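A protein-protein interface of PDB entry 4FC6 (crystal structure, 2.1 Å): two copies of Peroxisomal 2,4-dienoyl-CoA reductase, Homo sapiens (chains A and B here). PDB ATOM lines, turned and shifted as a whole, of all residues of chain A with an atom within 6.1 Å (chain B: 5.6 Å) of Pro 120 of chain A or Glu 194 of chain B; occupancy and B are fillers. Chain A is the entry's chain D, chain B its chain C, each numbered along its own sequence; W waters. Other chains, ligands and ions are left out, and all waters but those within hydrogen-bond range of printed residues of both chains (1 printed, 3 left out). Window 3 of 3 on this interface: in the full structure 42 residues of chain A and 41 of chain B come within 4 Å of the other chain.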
ATOM      1  N   LEU A 118     -23.586   6.439 -25.366  1.00  0.00           N
ATOM      2  CA  LEU A 118     -24.894   6.304 -24.728  1.00  0.00           C
ATOM      3  C   LEU A 118     -25.369   4.846 -24.777  1.00  0.00           C
ATOM      4  O   LEU A 118     -25.245   4.147 -25.787  1.00  0.00           O
ATOM      5  CB  LEU A 118     -25.942   7.230 -25.385  1.00  0.00           C
ATOM      6  CG  LEU A 118     -25.785   8.754 -25.420  1.00  0.00           C
ATOM      7  CD1 LEU A 118     -26.818   9.444 -26.363  1.00  0.00           C
ATOM      8  CD2 LEU A 118     -25.991   9.251 -23.986  1.00  0.00           C
ATOM      9  N   CYS A 119     -25.925   4.358 -23.697  1.00  0.00           N
ATOM     10  CA  CYS A 119     -26.495   3.014 -23.654  1.00  0.00           C
ATOM     11  C   CYS A 119     -27.291   2.738 -22.389  1.00  0.00           C
ATOM     12  O   CYS A 119     -26.808   2.965 -21.337  1.00  0.00           O
ATOM     13  CB  CYS A 119     -25.423   1.941 -23.843  1.00  0.00           C
ATOM     14  SG  CYS A 119     -25.854   0.212 -23.926  1.00  0.00           S
ATOM     15  N   PRO A 120     -28.510   2.233 -22.548  1.00  0.00           N
ATOM     16  CA  PRO A 120     -29.355   1.807 -21.417  1.00  0.00           C
ATOM     17  C   PRO A 120     -28.629   0.760 -20.600  1.00  0.00           C
ATOM     18  O   PRO A 120     -27.979  -0.141 -21.168  1.00  0.00           O
ATOM     19  CB  PRO A 120     -30.606   1.210 -22.105  1.00  0.00           C
ATOM     20  CG  PRO A 120     -30.618   1.819 -23.484  1.00  0.00           C
ATOM     21  CD  PRO A 120     -29.165   2.023 -23.861  1.00  0.00           C
ATOM     22  N   ALA A 121     -28.672   0.884 -19.267  1.00  0.00           N
ATOM     23  CA  ALA A 121     -27.934  -0.081 -18.406  1.00  0.00           C
ATOM     24  C   ALA A 121     -28.411  -1.510 -18.644  1.00  0.00           C
ATOM     25  O   ALA A 121     -27.635  -2.445 -18.543  1.00  0.00           O
ATOM     26  CB  ALA A 121     -28.079   0.282 -16.928  1.00  0.00           C
ATOM     27  N   GLY A 122     -29.703  -1.680 -18.924  1.00  0.00           N
ATOM     28  CA  GLY A 122     -30.240  -3.004 -19.199  1.00  0.00           C
ATOM     29  C   GLY A 122     -29.672  -3.612 -20.457  1.00  0.00           C
ATOM     30  O   GLY A 122     -29.747  -4.820 -20.609  1.00  0.00           O
ATOM     31  N   ALA A 123     -29.086  -2.789 -21.337  1.00  0.00           N
ATOM     32  CA  ALA A 123     -28.569  -3.246 -22.637  1.00  0.00           C
ATOM     33  C   ALA A 123     -27.035  -3.259 -22.720  1.00  0.00           C
ATOM     34  O   ALA A 123     -26.448  -3.757 -23.704  1.00  0.00           O
ATOM     35  CB  ALA A 123     -29.122  -2.351 -23.763  1.00  0.00           C
ATOM     36  N   LEU A 124     -26.384  -2.679 -21.714  1.00  0.00           N
ATOM     37  CA  LEU A 124     -24.942  -2.577 -21.664  1.00  0.00           C
ATOM     38  C   LEU A 124     -24.337  -3.957 -21.298  1.00  0.00           C
ATOM     39  O   LEU A 124     -24.775  -4.592 -20.313  1.00  0.00           O
ATOM     40  CB  LEU A 124     -24.608  -1.472 -20.621  1.00  0.00           C
ATOM     41  CG  LEU A 124     -23.159  -1.066 -20.390  1.00  0.00           C
ATOM     42  CD1 LEU A 124     -22.673  -0.210 -21.564  1.00  0.00           C
ATOM     43  CD2 LEU A 124     -23.020  -0.236 -19.116  1.00  0.00           C
ATOM     44  N   GLY A 170     -27.249  10.396 -11.472  1.00  0.00           N
ATOM     45  CA  GLY A 170     -27.478   9.099 -12.110  1.00  0.00           C
ATOM     46  C   GLY A 170     -28.048   9.323 -13.521  1.00  0.00           C
ATOM     47  O   GLY A 170     -29.144   8.772 -13.872  1.00  0.00           O
ATOM     48  N   GLN A 171     -27.337  10.138 -14.309  1.00  0.00           N
ATOM     49  CA  GLN A 171     -27.721  10.460 -15.685  1.00  0.00           C
ATOM     50  C   GLN A 171     -28.017   9.208 -16.489  1.00  0.00           C
ATOM     51  O   GLN A 171     -27.197   8.287 -16.552  1.00  0.00           O
ATOM     52  CB  GLN A 171     -26.605  11.261 -16.342  1.00  0.00           C
ATOM     53  CG  GLN A 171     -27.060  11.991 -17.597  1.00  0.00           C
ATOM     54  CD  GLN A 171     -28.247  12.906 -17.334  1.00  0.00           C
ATOM     55  OE1 GLN A 171     -28.309  13.627 -16.325  1.00  0.00           O
ATOM     56  NE2 GLN A 171     -29.221  12.839 -18.221  1.00  0.00           N
ATOM     57  N   ALA A 172     -29.224   9.137 -17.028  1.00  0.00           N
ATOM     58  CA  ALA A 172     -29.685   7.978 -17.795  1.00  0.00           C
ATOM     59  C   ALA A 172     -28.723   7.708 -18.909  1.00  0.00           C
ATOM     60  O   ALA A 172     -28.143   8.660 -19.447  1.00  0.00           O
ATOM     61  CB  ALA A 172     -31.058   8.272 -18.420  1.00  0.00           C
ATOM     62  N   LEU A 173     -28.579   6.427 -19.275  1.00  0.00           N
ATOM     63  CA  LEU A 173     -27.763   5.996 -20.434  1.00  0.00           C
ATOM     64  C   LEU A 173     -26.233   6.096 -20.174  1.00  0.00           C
ATOM     65  O   LEU A 173     -25.403   6.009 -21.086  1.00  0.00           O
ATOM     66  CB  LEU A 173     -28.146   6.798 -21.714  1.00  0.00           C
ATOM     67  CG  LEU A 173     -29.412   6.520 -22.585  1.00  0.00           C
ATOM     68  CD1 LEU A 173     -30.517   5.715 -21.902  1.00  0.00           C
ATOM     69  CD2 LEU A 173     -29.908   7.748 -23.350  1.00  0.00           C
ATOM     70  N   GLN A 174     -25.877   6.339 -18.924  1.00  0.00           N
ATOM     71  CA  GLN A 174     -24.495   6.671 -18.582  1.00  0.00           C
ATOM     72  C   GLN A 174     -23.997   5.921 -17.339  1.00  0.00           C
ATOM     73  O   GLN A 174     -23.088   6.404 -16.658  1.00  0.00           O
ATOM     74  CB  GLN A 174     -24.403   8.186 -18.369  1.00  0.00           C
ATOM     75  CG  GLN A 174     -24.573   9.036 -19.611  1.00  0.00           C
ATOM     76  CD  GLN A 174     -23.383   8.871 -20.518  1.00  0.00           C
ATOM     77  OE1 GLN A 174     -23.273   7.859 -21.222  1.00  0.00           O
ATOM     78  NE2 GLN A 174     -22.472   9.807 -20.476  1.00  0.00           N
ATOM     79  N   VAL A 175     -24.561   4.764 -17.025  1.00  0.00           N
ATOM     80  CA  VAL A 175     -24.186   4.093 -15.744  1.00  0.00           C
ATOM     81  C   VAL A 175     -22.646   3.834 -15.684  1.00  0.00           C
ATOM     82  O   VAL A 175     -21.979   4.088 -14.670  1.00  0.00           O
ATOM     83  CB  VAL A 175     -24.999   2.805 -15.465  1.00  0.00           C
ATOM     84  CG1 VAL A 175     -24.728   1.716 -16.537  1.00  0.00           C
ATOM     85  CG2 VAL A 175     -24.691   2.302 -14.062  1.00  0.00           C
ATOM     86  N   ARG B 189     -27.725   5.370  -7.948  1.00  0.00           N
ATOM     87  CA  ARG B 189     -28.451   6.448  -8.543  1.00  0.00           C
ATOM     88  C   ARG B 189     -28.848   6.170  -9.995  1.00  0.00           C
ATOM     89  O   ARG B 189     -29.959   6.346 -10.328  1.00  0.00           O
ATOM     90  CB  ARG B 189     -27.714   7.762  -8.378  1.00  0.00           C
ATOM     91  CG  ARG B 189     -27.817   8.293  -6.955  1.00  0.00           C
ATOM     92  CD  ARG B 189     -27.170   9.611  -6.658  1.00  0.00           C
ATOM     93  NE  ARG B 189     -25.765   9.602  -6.854  1.00  0.00           N
ATOM     94  CZ  ARG B 189     -24.842   9.195  -6.004  1.00  0.00           C
ATOM     95  NH1 ARG B 189     -23.601   9.260  -6.388  1.00  0.00           N
ATOM     96  NH2 ARG B 189     -25.123   8.757  -4.812  1.00  0.00           N
ATOM     97  N   HIS B 190     -27.889   5.709 -10.783  1.00  0.00           N
ATOM     98  CA  HIS B 190     -28.058   5.379 -12.180  1.00  0.00           C
ATOM     99  C   HIS B 190     -29.128   4.304 -12.396  1.00  0.00           C
ATOM    100  O   HIS B 190     -30.002   4.507 -13.185  1.00  0.00           O
ATOM    101  CB  HIS B 190     -26.746   4.962 -12.848  1.00  0.00           C
ATOM    102  CG  HIS B 190     -25.822   6.100 -13.208  1.00  0.00           C
ATOM    103  ND1 HIS B 190     -26.003   6.863 -14.259  1.00  0.00           N
ATOM    104  CD2 HIS B 190     -24.661   6.522 -12.634  1.00  0.00           C
ATOM    105  CE1 HIS B 190     -25.038   7.740 -14.344  1.00  0.00           C
ATOM    106  NE2 HIS B 190     -24.207   7.529 -13.361  1.00  0.00           N
ATOM    107  N   LEU B 191     -29.061   3.200 -11.678  1.00  0.00           N
ATOM    108  CA  LEU B 191     -30.016   2.143 -11.833  1.00  0.00           C
ATOM    109  C   LEU B 191     -31.385   2.557 -11.290  1.00  0.00           C
ATOM    110  O   LEU B 191     -32.387   2.170 -11.846  1.00  0.00           O
ATOM    111  CB  LEU B 191     -29.545   0.828 -11.163  1.00  0.00           C
ATOM    112  CG  LEU B 191     -28.264   0.310 -11.856  1.00  0.00           C
ATOM    113  CD1 LEU B 191     -27.568  -0.879 -11.207  1.00  0.00           C
ATOM    114  CD2 LEU B 191     -28.427   0.069 -13.376  1.00  0.00           C
ATOM    115  N   ALA B 192     -31.427   3.329 -10.212  1.00  0.00           N
ATOM    116  CA  ALA B 192     -32.718   3.739  -9.658  1.00  0.00           C
ATOM    117  C   ALA B 192     -33.450   4.572 -10.671  1.00  0.00           C
ATOM    118  O   ALA B 192     -34.693   4.405 -10.832  1.00  0.00           O
ATOM    119  CB  ALA B 192     -32.569   4.519  -8.361  1.00  0.00           C
ATOM    120  N   VAL B 193     -32.712   5.443 -11.360  1.00  0.00           N
ATOM    121  CA  VAL B 193     -33.308   6.284 -12.397  1.00  0.00           C
ATOM    122  C   VAL B 193     -33.803   5.398 -13.570  1.00  0.00           C
ATOM    123  O   VAL B 193     -34.937   5.533 -14.005  1.00  0.00           O
ATOM    124  CB  VAL B 193     -32.356   7.391 -12.868  1.00  0.00           C
ATOM    125  CG1 VAL B 193     -32.795   8.045 -14.205  1.00  0.00           C
ATOM    126  CG2 VAL B 193     -32.167   8.442 -11.753  1.00  0.00           C
ATOM    127  N   GLU B 194     -33.002   4.456 -14.058  1.00  0.00           N
ATOM    128  CA  GLU B 194     -33.392   3.772 -15.303  1.00  0.00           C
ATOM    129  C   GLU B 194     -34.414   2.668 -15.010  1.00  0.00           C
ATOM    130  O   GLU B 194     -35.272   2.448 -15.827  1.00  0.00           O
ATOM    131  CB  GLU B 194     -32.154   3.167 -16.009  1.00  0.00           C
ATOM    132  CG  GLU B 194     -31.296   4.235 -16.699  1.00  0.00           C
ATOM    133  CD  GLU B 194     -30.327   3.626 -17.699  1.00  0.00           C
ATOM    134  OE1 GLU B 194     -30.646   2.559 -18.258  1.00  0.00           O
ATOM    135  OE2 GLU B 194     -29.236   4.209 -17.931  1.00  0.00           O
ATOM    136  N   TRP B 195     -34.324   2.031 -13.836  1.00  0.00           N
ATOM    137  CA  TRP B 195     -35.086   0.840 -13.522  1.00  0.00           C
ATOM    138  C   TRP B 195     -36.290   1.082 -12.666  1.00  0.00           C
ATOM    139  O   TRP B 195     -37.155   0.186 -12.508  1.00  0.00           O
ATOM    140  CB  TRP B 195     -34.159  -0.244 -12.915  1.00  0.00           C
ATOM    141  CG  TRP B 195     -33.113  -0.718 -13.909  1.00  0.00           C
ATOM    142  CD1 TRP B 195     -33.002  -0.355 -15.269  1.00  0.00           C
ATOM    143  CD2 TRP B 195     -32.033  -1.646 -13.669  1.00  0.00           C
ATOM    144  NE1 TRP B 195     -31.991  -0.991 -15.862  1.00  0.00           N
ATOM    145  CE2 TRP B 195     -31.356  -1.815 -14.948  1.00  0.00           C
ATOM    146  CE3 TRP B 195     -31.606  -2.383 -12.565  1.00  0.00           C
ATOM    147  CZ2 TRP B 195     -30.252  -2.630 -15.086  1.00  0.00           C
ATOM    148  CZ3 TRP B 195     -30.522  -3.230 -12.715  1.00  0.00           C
ATOM    149  CH2 TRP B 195     -29.842  -3.346 -13.953  1.00  0.00           C
ATOM    150  N   GLY B 196     -36.386   2.292 -12.116  1.00  0.00           N
ATOM    151  CA  GLY B 196     -37.581   2.740 -11.364  1.00  0.00           C
ATOM    152  C   GLY B 196     -38.878   2.389 -12.108  1.00  0.00           C
ATOM    153  O   GLY B 196     -39.789   1.811 -11.503  1.00  0.00           O
ATOM    154  N   PRO B 197     -38.970   2.724 -13.423  1.00  0.00           N
ATOM    155  CA  PRO B 197     -40.245   2.461 -14.162  1.00  0.00           C
ATOM    156  C   PRO B 197     -40.576   0.986 -14.306  1.00  0.00           C
ATOM    157  O   PRO B 197     -41.724   0.625 -14.561  1.00  0.00           O
ATOM    158  CB  PRO B 197     -39.982   3.083 -15.546  1.00  0.00           C
ATOM    159  CG  PRO B 197     -39.078   4.256 -15.223  1.00  0.00           C
ATOM    160  CD  PRO B 197     -38.134   3.712 -14.138  1.00  0.00           C
ATOM    161  N   GLN B 198     -39.602   0.125 -14.059  1.00  0.00           N
ATOM    162  CA  GLN B 198     -39.862  -1.280 -14.105  1.00  0.00           C
ATOM    163  C   GLN B 198     -40.212  -1.788 -12.752  1.00  0.00           C
ATOM    164  O   GLN B 198     -40.172  -2.998 -12.534  1.00  0.00           O
ATOM    165  CB  GLN B 198     -38.648  -2.031 -14.614  1.00  0.00           C
ATOM    166  CG  GLN B 198     -38.762  -2.258 -16.081  1.00  0.00           C
ATOM    167  CD  GLN B 198     -38.323  -1.047 -16.802  1.00  0.00           C
ATOM    168  OE1 GLN B 198     -39.143  -0.293 -17.339  1.00  0.00           O
ATOM    169  NE2 GLN B 198     -37.013  -0.799 -16.774  1.00  0.00           N
HETATM  170  O   HOH W   1     -27.830   5.296 -16.144  1.00  0.00           O
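Water W1 lies within hydrogen-bond range of OE2 of Glu 194 of chain B (2.5 Å), ND1 of His 190 of chain B (3.1 Å), O of Gln 171 of chain A (3.1 Å), N of Leu 173 of chain A (3.4 Å) and N of Val 175 of chain A (3.4 Å).
Of the printed residues of chain B, Pro 120 of chain A touches Glu 194.
Printed residues of chain B within 4 Å of Ala 121 of chain A: Leu 191 (3.6 Å) and Glu 194 (2.8 Å).
Printed residues of chain B within 4 Å of Gly 122 of chain A: Trp 195 (3.9 Å).
Of the printed residues of chain A, Arg 189 of chain B touches Gly 170.
Glu 194 of chain B touches just these residues of chain A: Pro 120, Ala 121, Ala 172 and Leu 173.
The nearest printed residue of chain B that does not touch Pro 120 of chain A is Trp 195 of chain B (6.1 Å).
The nearest residue of chain A that does not touch Glu 194 of chain B is Gln 174 of chain A (4.1 Å).
No position is printed for both chains.
Of the 12 pairs that touch across the chains among the printed residues, none has its exchanged pair printed and touching as well.
Of the 10 printed residues of chain B, 6 touch a printed residue of chain A.
Printed residues of chain B that touch a printed residue of chain A: Arg 189, His 190, Leu 191, Val 193, Glu 194 and Trp 195.
Hydrophobic or aromatic side chains of chain A that line the printed part of chain B: Ala 121 and Val 175.
Among the printed residues, no Asp or Glu carboxylate lies within 4 Å of a Lys or Arg side-chain nitrogen of the other chain.
The backbone carbonyl oxygen of Leu 173 of chain A lies within hydrogen-bond range of the backbone NH of Cys 119 of chain A, 3.1 Å away.
OE1 of Glu 194 of chain B touches CA of Pro 120 of chain A, 3.5 Å away.
Leu 191 of chain B touches Ala 121 of chain A.
Gly 122 of chain A touches Trp 195 of chain B (N to NE1, 3.9 Å).
Gly 170 of chain A touches Arg 189 of chain B.
C of Gly 170 of chain A touches ND1 of His 190 of chain B, 3.3 Å away.
Gly 170 of chain A touches Val 193 of chain B.
Ala 172 of chain A touches Glu 194 of chain B (C to OE2, 3.7 Å).
Gln 174 of chain A touches His 190 of chain B.
Val 175 of chain A touches His 190 of chain B (CG2 to CB, 3.6 Å).
A ring nitrogen (ND1) of His 190 of chain B sits at hydrogen-bond distance from the backbone carbonyl oxygen (O) of Gln 171 of chain A (3.0 Å).
The side-chain carboxylate (OE1) of Glu 194 of chain B lies within hydrogen-bond range of the backbone NH (N) of Ala 121 of chain A, at 2.8 Å.
The side-chain carboxylate of Glu 194 of chain B lies within hydrogen-bond range of the backbone NH of Leu 173 of chain A (2.7 Å).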
